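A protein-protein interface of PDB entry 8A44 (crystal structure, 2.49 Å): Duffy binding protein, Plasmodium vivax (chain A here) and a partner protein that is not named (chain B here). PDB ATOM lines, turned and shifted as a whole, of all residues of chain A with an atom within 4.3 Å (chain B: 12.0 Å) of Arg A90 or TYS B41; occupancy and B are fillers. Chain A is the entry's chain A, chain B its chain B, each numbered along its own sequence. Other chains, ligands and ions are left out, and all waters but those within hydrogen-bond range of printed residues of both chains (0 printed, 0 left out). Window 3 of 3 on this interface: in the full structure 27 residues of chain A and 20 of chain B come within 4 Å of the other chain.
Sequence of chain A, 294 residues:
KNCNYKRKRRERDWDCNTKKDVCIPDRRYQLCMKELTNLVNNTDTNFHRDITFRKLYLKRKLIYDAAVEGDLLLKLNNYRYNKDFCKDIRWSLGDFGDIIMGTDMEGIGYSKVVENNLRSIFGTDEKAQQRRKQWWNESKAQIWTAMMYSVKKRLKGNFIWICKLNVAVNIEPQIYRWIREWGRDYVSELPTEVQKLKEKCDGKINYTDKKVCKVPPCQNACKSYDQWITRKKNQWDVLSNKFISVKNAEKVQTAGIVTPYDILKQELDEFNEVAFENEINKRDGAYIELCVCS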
ATOM      1  N   LYS A  83       8.863   5.406 -29.887  1.00  0.00           N
ATOM      2  CA  LYS A  83      10.119   6.109 -30.120  1.00  0.00           C
ATOM      3  C   LYS A  83      10.214   6.690 -31.531  1.00  0.00           C
ATOM      4  O   LYS A  83      10.875   7.715 -31.726  1.00  0.00           O
ATOM      5  CB  LYS A  83      11.280   5.155 -29.814  1.00  0.00           C
ATOM      6  CG  LYS A  83      12.388   5.089 -30.849  1.00  0.00           C
ATOM      7  CD  LYS A  83      13.643   4.450 -30.254  1.00  0.00           C
ATOM      8  CE  LYS A  83      13.673   2.937 -30.465  1.00  0.00           C
ATOM      9  NZ  LYS A  83      14.855   2.305 -29.808  1.00  0.00           N
ATOM     10  N   CYS A  86       8.650  10.124 -31.242  1.00  0.00           N
ATOM     11  CA  CYS A  86       9.602  10.996 -30.556  1.00  0.00           C
ATOM     12  C   CYS A  86      10.712  11.487 -31.482  1.00  0.00           C
ATOM     13  O   CYS A  86      11.048  12.680 -31.481  1.00  0.00           O
ATOM     14  CB  CYS A  86      10.182  10.256 -29.352  1.00  0.00           C
ATOM     15  SG  CYS A  86       8.902   9.920 -28.099  1.00  0.00           S
ATOM     16  N   LYS A  87      11.290  10.591 -32.286  1.00  0.00           N
ATOM     17  CA  LYS A  87      12.339  11.014 -33.211  1.00  0.00           C
ATOM     18  C   LYS A  87      11.819  12.057 -34.204  1.00  0.00           C
ATOM     19  O   LYS A  87      12.466  13.091 -34.426  1.00  0.00           O
ATOM     20  CB  LYS A  87      12.913   9.797 -33.936  1.00  0.00           C
ATOM     21  CG  LYS A  87      13.566   8.770 -33.002  1.00  0.00           C
ATOM     22  CD  LYS A  87      14.961   9.197 -32.518  1.00  0.00           C
ATOM     23  CE  LYS A  87      15.713   8.010 -31.919  1.00  0.00           C
ATOM     24  NZ  LYS A  87      17.067   8.372 -31.434  1.00  0.00           N
ATOM     25  N   ASP A  88      10.635  11.824 -34.779  1.00  0.00           N
ATOM     26  CA  ASP A  88      10.039  12.814 -35.674  1.00  0.00           C
ATOM     27  C   ASP A  88       9.831  14.156 -34.978  1.00  0.00           C
ATOM     28  O   ASP A  88      10.136  15.214 -35.551  1.00  0.00           O
ATOM     29  CB  ASP A  88       8.714  12.299 -36.221  1.00  0.00           C
ATOM     30  CG  ASP A  88       8.884  11.565 -37.536  1.00  0.00           C
ATOM     31  OD1 ASP A  88      10.015  11.102 -37.842  1.00  0.00           O
ATOM     32  OD2 ASP A  88       7.881  11.462 -38.269  1.00  0.00           O
ATOM     33  N   ILE A  89       9.292  14.136 -33.754  1.00  0.00           N
ATOM     34  CA  ILE A  89       9.116  15.378 -33.005  1.00  0.00           C
ATOM     35  C   ILE A  89      10.456  16.087 -32.867  1.00  0.00           C
ATOM     36  O   ILE A  89      10.564  17.302 -33.083  1.00  0.00           O
ATOM     37  CB  ILE A  89       8.474  15.097 -31.629  1.00  0.00           C
ATOM     38  CG1 ILE A  89       6.997  14.692 -31.770  1.00  0.00           C
ATOM     39  CG2 ILE A  89       8.581  16.334 -30.713  1.00  0.00           C
ATOM     40  CD1 ILE A  89       6.152  15.690 -32.553  1.00  0.00           C
ATOM     41  N   ARG A  90      11.511  15.322 -32.558  1.00  0.00           N
ATOM     42  CA  ARG A  90      12.837  15.906 -32.421  1.00  0.00           C
ATOM     43  C   ARG A  90      13.329  16.494 -33.747  1.00  0.00           C
ATOM     44  O   ARG A  90      13.900  17.595 -33.766  1.00  0.00           O
ATOM     45  CB  ARG A  90      13.795  14.845 -31.876  1.00  0.00           C
ATOM     46  CG  ARG A  90      15.252  15.252 -31.751  1.00  0.00           C
ATOM     47  CD  ARG A  90      16.013  14.220 -30.942  1.00  0.00           C
ATOM     48  NE  ARG A  90      17.454  14.278 -31.166  1.00  0.00           N
ATOM     49  CZ  ARG A  90      18.282  13.259 -30.977  1.00  0.00           C
ATOM     50  NH1 ARG A  90      17.848  12.083 -30.553  1.00  0.00           N
ATOM     51  NH2 ARG A  90      19.579  13.421 -31.232  1.00  0.00           N
ATOM     52  N   TRP A  91      13.091  15.799 -34.867  1.00  0.00           N
ATOM     53  CA  TRP A  91      13.608  16.275 -36.149  1.00  0.00           C
ATOM     54  C   TRP A  91      12.905  17.546 -36.605  1.00  0.00           C
ATOM     55  O   TRP A  91      13.549  18.449 -37.155  1.00  0.00           O
ATOM     56  CB  TRP A  91      13.479  15.195 -37.226  1.00  0.00           C
ATOM     57  CG  TRP A  91      14.100  13.826 -36.912  1.00  0.00           C
ATOM     58  CD1 TRP A  91      13.663  12.610 -37.376  1.00  0.00           C
ATOM     59  CD2 TRP A  91      15.251  13.546 -36.091  1.00  0.00           C
ATOM     60  NE1 TRP A  91      14.465  11.602 -36.900  1.00  0.00           N
ATOM     61  CE2 TRP A  91      15.441  12.148 -36.103  1.00  0.00           C
ATOM     62  CE3 TRP A  91      16.128  14.335 -35.339  1.00  0.00           C
ATOM     63  CZ2 TRP A  91      16.466  11.525 -35.389  1.00  0.00           C
ATOM     64  CZ3 TRP A  91      17.153  13.712 -34.640  1.00  0.00           C
ATOM     65  CH2 TRP A  91      17.311  12.322 -34.672  1.00  0.00           C
ATOM     66  N   SER A  92      11.584  17.629 -36.408  1.00  0.00           N
ATOM     67  CA  SER A  92      10.850  18.818 -36.834  1.00  0.00           C
ATOM     68  C   SER A  92      11.082  19.998 -35.890  1.00  0.00           C
ATOM     69  O   SER A  92      11.184  21.142 -36.347  1.00  0.00           O
ATOM     70  CB  SER A  92       9.354  18.513 -36.954  1.00  0.00           C
ATOM     71  OG  SER A  92       9.075  17.866 -38.183  1.00  0.00           O
ATOM     72  N   LEU A  93      11.149  19.763 -34.575  1.00  0.00           N
ATOM     73  CA  LEU A  93      11.556  20.845 -33.676  1.00  0.00           C
ATOM     74  C   LEU A  93      12.905  21.420 -34.104  1.00  0.00           C
ATOM     75  O   LEU A  93      13.059  22.642 -34.237  1.00  0.00           O
ATOM     76  CB  LEU A  93      11.615  20.358 -32.226  1.00  0.00           C
ATOM     77  CG  LEU A  93      12.091  21.406 -31.205  1.00  0.00           C
ATOM     78  CD1 LEU A  93      11.078  22.515 -31.129  1.00  0.00           C
ATOM     79  CD2 LEU A  93      12.298  20.797 -29.816  1.00  0.00           C
ATOM     80  N   GLY A  94      13.880  20.540 -34.377  1.00  0.00           N
ATOM     81  CA  GLY A  94      15.184  21.001 -34.832  1.00  0.00           C
ATOM     82  C   GLY A  94      15.108  21.837 -36.096  1.00  0.00           C
ATOM     83  O   GLY A  94      15.871  22.795 -36.271  1.00  0.00           O
ATOM     84  N   ILE A 162       7.662   9.556 -22.637  1.00  0.00           N
ATOM     85  CA  ILE A 162       8.520   8.712 -23.458  1.00  0.00           C
ATOM     86  C   ILE A 162       9.613   9.550 -24.107  1.00  0.00           C
ATOM     87  O   ILE A 162      10.810   9.314 -23.901  1.00  0.00           O
ATOM     88  CB  ILE A 162       7.691   7.953 -24.507  1.00  0.00           C
ATOM     89  CG1 ILE A 162       6.684   7.026 -23.825  1.00  0.00           C
ATOM     90  CG2 ILE A 162       8.601   7.154 -25.426  1.00  0.00           C
ATOM     91  CD1 ILE A 162       6.119   5.986 -24.745  1.00  0.00           C
ATOM     92  N   LYS A 164      12.080  12.580 -24.389  1.00  0.00           N
ATOM     93  CA  LYS A 164      12.857  13.259 -23.362  1.00  0.00           C
ATOM     94  C   LYS A 164      13.170  14.678 -23.832  1.00  0.00           C
ATOM     95  O   LYS A 164      13.753  14.869 -24.905  1.00  0.00           O
ATOM     96  CB  LYS A 164      14.128  12.468 -23.038  1.00  0.00           C
ATOM     97  CG  LYS A 164      14.417  11.314 -24.019  1.00  0.00           C
ATOM     98  CD  LYS A 164      15.532  10.395 -23.514  1.00  0.00           C
ATOM     99  CE  LYS A 164      15.714   9.171 -24.390  1.00  0.00           C
ATOM    100  NZ  LYS A 164      16.763   8.265 -23.848  1.00  0.00           N
ATOM    101  N   VAL A 167      16.925  15.683 -24.695  1.00  0.00           N
ATOM    102  CA  VAL A 167      17.428  15.194 -25.980  1.00  0.00           C
ATOM    103  C   VAL A 167      16.885  16.040 -27.133  1.00  0.00           C
ATOM    104  O   VAL A 167      17.628  16.426 -28.049  1.00  0.00           O
ATOM    105  CB  VAL A 167      17.083  13.702 -26.161  1.00  0.00           C
ATOM    106  CG1 VAL A 167      17.172  13.300 -27.625  1.00  0.00           C
ATOM    107  CG2 VAL A 167      17.994  12.831 -25.321  1.00  0.00           C
ATOM    108  N   ALA A 168      15.586  16.371 -27.092  1.00  0.00           N
ATOM    109  CA  ALA A 168      14.945  17.029 -28.232  1.00  0.00           C
ATOM    110  C   ALA A 168      15.422  18.473 -28.422  1.00  0.00           C
ATOM    111  O   ALA A 168      15.558  18.940 -29.559  1.00  0.00           O
ATOM    112  CB  ALA A 168      13.428  16.993 -28.072  1.00  0.00           C
ATOM    113  N   ARG A 180      21.288  11.560 -38.753  1.00  0.00           N
ATOM    114  CA  ARG A 180      20.595  10.693 -37.805  1.00  0.00           C
ATOM    115  C   ARG A 180      19.303  10.170 -38.411  1.00  0.00           C
ATOM    116  O   ARG A 180      19.034   8.960 -38.388  1.00  0.00           O
ATOM    117  CB  ARG A 180      20.290  11.441 -36.511  1.00  0.00           C
ATOM    118  CG  ARG A 180      21.475  11.971 -35.748  1.00  0.00           C
ATOM    119  CD  ARG A 180      20.986  12.597 -34.460  1.00  0.00           C
ATOM    120  NE  ARG A 180      22.034  13.312 -33.747  1.00  0.00           N
ATOM    121  CZ  ARG A 180      22.964  12.720 -33.013  1.00  0.00           C
ATOM    122  NH1 ARG A 180      23.027  11.402 -32.903  1.00  0.00           N
ATOM    123  NH2 ARG A 180      23.852  13.469 -32.371  1.00  0.00           N
ATOM    124  N   PRO B  37       4.891  10.619 -15.050  1.00  0.00           N
ATOM    125  CA  PRO B  37       6.168   9.930 -14.827  1.00  0.00           C
ATOM    126  C   PRO B  37       6.940   9.671 -16.116  1.00  0.00           C
ATOM    127  O   PRO B  37       6.419   9.786 -17.225  1.00  0.00           O
ATOM    128  CB  PRO B  37       5.733   8.593 -14.181  1.00  0.00           C
ATOM    129  CG  PRO B  37       4.295   8.370 -14.650  1.00  0.00           C
ATOM    130  CD  PRO B  37       3.852   9.631 -15.432  1.00  0.00           C
ATOM    131  N   ASP B  38       8.219   9.361 -15.938  1.00  0.00           N
ATOM    132  CA  ASP B  38       9.064   9.042 -17.073  1.00  0.00           C
ATOM    133  C   ASP B  38       8.683   7.681 -17.619  1.00  0.00           C
ATOM    134  O   ASP B  38       8.332   6.766 -16.868  1.00  0.00           O
ATOM    135  CB  ASP B  38      10.540   9.060 -16.677  1.00  0.00           C
ATOM    136  CG  ASP B  38      11.163  10.425 -16.876  1.00  0.00           C
ATOM    137  OD1 ASP B  38      10.916  11.026 -17.946  1.00  0.00           O
ATOM    138  OD2 ASP B  38      11.893  10.894 -15.970  1.00  0.00           O
ATOM    139  N   GLY B  39       8.754   7.567 -18.937  1.00  0.00           N
ATOM    140  CA  GLY B  39       8.487   6.272 -19.570  1.00  0.00           C
ATOM    141  C   GLY B  39       9.760   5.755 -20.196  1.00  0.00           C
ATOM    142  O   GLY B  39      10.636   6.571 -20.514  1.00  0.00           O
ATOM    143  N   ASP B  40       9.850   4.435 -20.368  1.00  0.00           N
ATOM    144  CA  ASP B  40      11.030   3.828 -21.030  1.00  0.00           C
ATOM    145  C   ASP B  40      10.911   4.086 -22.525  1.00  0.00           C
ATOM    146  O   ASP B  40       9.811   3.924 -23.067  1.00  0.00           O
ATOM    147  CB  ASP B  40      11.153   2.334 -20.717  1.00  0.00           C
ATOM    148  CG  ASP B  40      11.562   1.501 -21.920  1.00  0.00           C
ATOM    149  OD1 ASP B  40      12.778   1.309 -22.113  1.00  0.00           O
ATOM    150  OD2 ASP B  40      10.661   1.055 -22.657  1.00  0.00           O
ATOM    151  N   TYS B  41      12.011   4.460 -23.168  1.00  0.00           N
ATOM    152  CA  TYS B  41      11.954   4.811 -24.558  1.00  0.00           C
ATOM    153  CB  TYS B  41      13.349   5.188 -25.051  1.00  0.00           C
ATOM    154  CG  TYS B  41      13.434   6.268 -26.052  1.00  0.00           C
ATOM    155  CD1 TYS B  41      14.450   6.228 -27.001  1.00  0.00           C
ATOM    156  CD2 TYS B  41      12.523   7.325 -26.058  1.00  0.00           C
ATOM    157  CE1 TYS B  41      14.574   7.219 -27.956  1.00  0.00           C
ATOM    158  CE2 TYS B  41      12.626   8.329 -27.005  1.00  0.00           C
ATOM    159  CZ  TYS B  41      13.651   8.272 -27.966  1.00  0.00           C
ATOM    160  OH  TYS B  41      13.746   9.252 -28.861  1.00  0.00           O
ATOM    161  S   TYS B  41      14.956  10.495 -28.842  1.00  0.00           S
ATOM    162  O1  TYS B  41      14.438  11.411 -29.733  1.00  0.00           O
ATOM    163  O2  TYS B  41      14.881  10.814 -27.499  1.00  0.00           O
ATOM    164  O3  TYS B  41      16.112   9.852 -29.235  1.00  0.00           O
ATOM    165  C   TYS B  41      11.411   3.723 -25.514  1.00  0.00           C
ATOM    166  O   TYS B  41      11.081   4.045 -26.682  1.00  0.00           O
ATOM    167  N   ASP B  42      11.322   2.483 -25.037  1.00  0.00           N
ATOM    168  CA  ASP B  42      10.884   1.379 -25.933  1.00  0.00           C
ATOM    169  C   ASP B  42       9.385   1.148 -25.744  1.00  0.00           C
ATOM    170  O   ASP B  42       8.849   0.235 -26.382  1.00  0.00           O
ATOM    171  CB  ASP B  42      11.720   0.120 -25.712  1.00  0.00           C
ATOM    172  CG  ASP B  42      13.204   0.408 -25.585  1.00  0.00           C
ATOM    173  OD1 ASP B  42      13.881  -0.334 -24.850  1.00  0.00           O
ATOM    174  OD2 ASP B  42      13.668   1.373 -26.220  1.00  0.00           O
ATOM    175  N   ALA B  43       8.758   1.981 -24.922  1.00  0.00           N
ATOM    176  CA  ALA B  43       7.310   1.848 -24.674  1.00  0.00           C
ATOM    177  C   ALA B  43       6.533   2.135 -25.954  1.00  0.00           C
ATOM    178  O   ALA B  43       7.126   2.648 -26.912  1.00  0.00           O
ATOM    179  CB  ALA B  43       6.898   2.762 -23.557  1.00  0.00           C
ATOM    180  N   ASN B  44       5.241   1.836 -25.941  1.00  0.00           N
ATOM    181  CA  ASN B  44       4.414   1.977 -27.135  1.00  0.00           C
ATOM    182  C   ASN B  44       2.946   2.001 -26.695  1.00  0.00           C
ATOM    183  O   ASN B  44       2.383   0.946 -26.392  1.00  0.00           O
ATOM    184  CB  ASN B  44       4.690   0.827 -28.085  1.00  0.00           C
ATOM    185  CG  ASN B  44       4.204   1.102 -29.480  1.00  0.00           C
ATOM    186  OD1 ASN B  44       3.022   1.343 -29.705  1.00  0.00           O
ATOM    187  ND2 ASN B  44       5.109   1.004 -30.442  1.00  0.00           N
ATOM    188  N   LEU B  45       2.358   3.199 -26.740  1.00  0.00           N
ATOM    189  CA  LEU B  45       0.948   3.364 -26.310  1.00  0.00           C
ATOM    190  C   LEU B  45       0.081   3.774 -27.503  1.00  0.00           C
ATOM    191  O   LEU B  45       0.580   3.801 -28.673  1.00  0.00           O
ATOM    192  CB  LEU B  45       0.891   4.440 -25.219  1.00  0.00           C
ATOM    193  CG  LEU B  45       1.604   4.102 -23.911  1.00  0.00           C
ATOM    194  CD1 LEU B  45       1.535   2.613 -23.616  1.00  0.00           C
ATOM    195  CD2 LEU B  45       3.048   4.579 -23.938  1.00  0.00           C
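The side-chain amino group of Lys A83 lies within salt-bridge range of the side-chain carboxylate of Asp B42, at 3.9 Å.
NZ of Lys A87 sits close to O3 of TYS B41 (2.8 Å).
O3 of TYS B41 sits close to the guanidinium group of Arg A90.
The side-chain carboxylate (OD2) of Asp B40 lies within hydrogen-bond range of the backbone NH (N) of Asp B42, 2.9 Å away.
The backbone NH (N) of Ala B43 lies within hydrogen-bond range of the side-chain carboxylate (OD2) of Asp B40, at 3.1 Å.
Among the printed residues, pairs that only touch across the chains: Lys A83 with TYS B41 (3.3 Å), Cys A86 with TYS B41 (3.7 Å), Ile A162 with TYS B41 (3.4 Å), Ile A162 with Ala B43 (3.5 Å), Ile A162 with Leu B45 (3.5 Å), Lys A164 with TYS B41 (3.5 Å) and Val A167 with TYS B41 (3.4 Å).
Lys A83 touches just these residues of chain B: TYS B41 (3.3 Å) and Asp B42 (3.9 Å).
Cys A86 touches just one residue of chain B: TYS B41 (3.7 Å).
No residue of chain B comes within 4 Å of Asp A88.
No residue of chain B comes within 4 Å of Ile A89.
No residue of chain B comes within 4 Å of Trp A91.
No residue of chain B comes within 4 Å of Ser A92.
No residue of chain B comes within 4 Å of Leu A93.
No residue of chain B comes within 4 Å of Gly A94.
Lys A164 touches just one residue of chain B: TYS B41.
Of chain B, only TYS B41 (3.4 Å) comes within 4 Å of Val A167.
No residue of chain B comes within 4 Å of Ala A168.
TYS B41 touches seven residues of chain A.
Of the printed residues of chain A, Asp B42 touches Lys A83.
Printed residues of chain A within 4 Å of Ala B43: Ile A162 (3.5 Å).
Of the printed residues of chain A, Leu B45 touches Ile A162.
The nearest printed residue of chain A that does not touch TYS B41 is Ala A168 (5.6 Å).
The nearest printed residue of chain A that does not touch Leu B45 is Lys A83 (7.6 Å).
Printed residues of chain A that touch a printed residue of chain B: Lys A83, Cys A86, Lys A87, Arg A90, Ile A162, Lys A164 and Val A167.
Hydrophobic or aromatic side chains of chain A that line the printed part of chain B: Ile A162 and Val A167.
Hydrophobic or aromatic side chains of chain B that line the printed part of chain A: Ala B43 and Leu B45.
Among the printed residues, 10 pairs touch across the chains.
Among the printed residues, Asp or Glu carboxylates within 4 Å of a Lys or Arg side-chain nitrogen of the other chain: Lys A83 with Asp B42.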
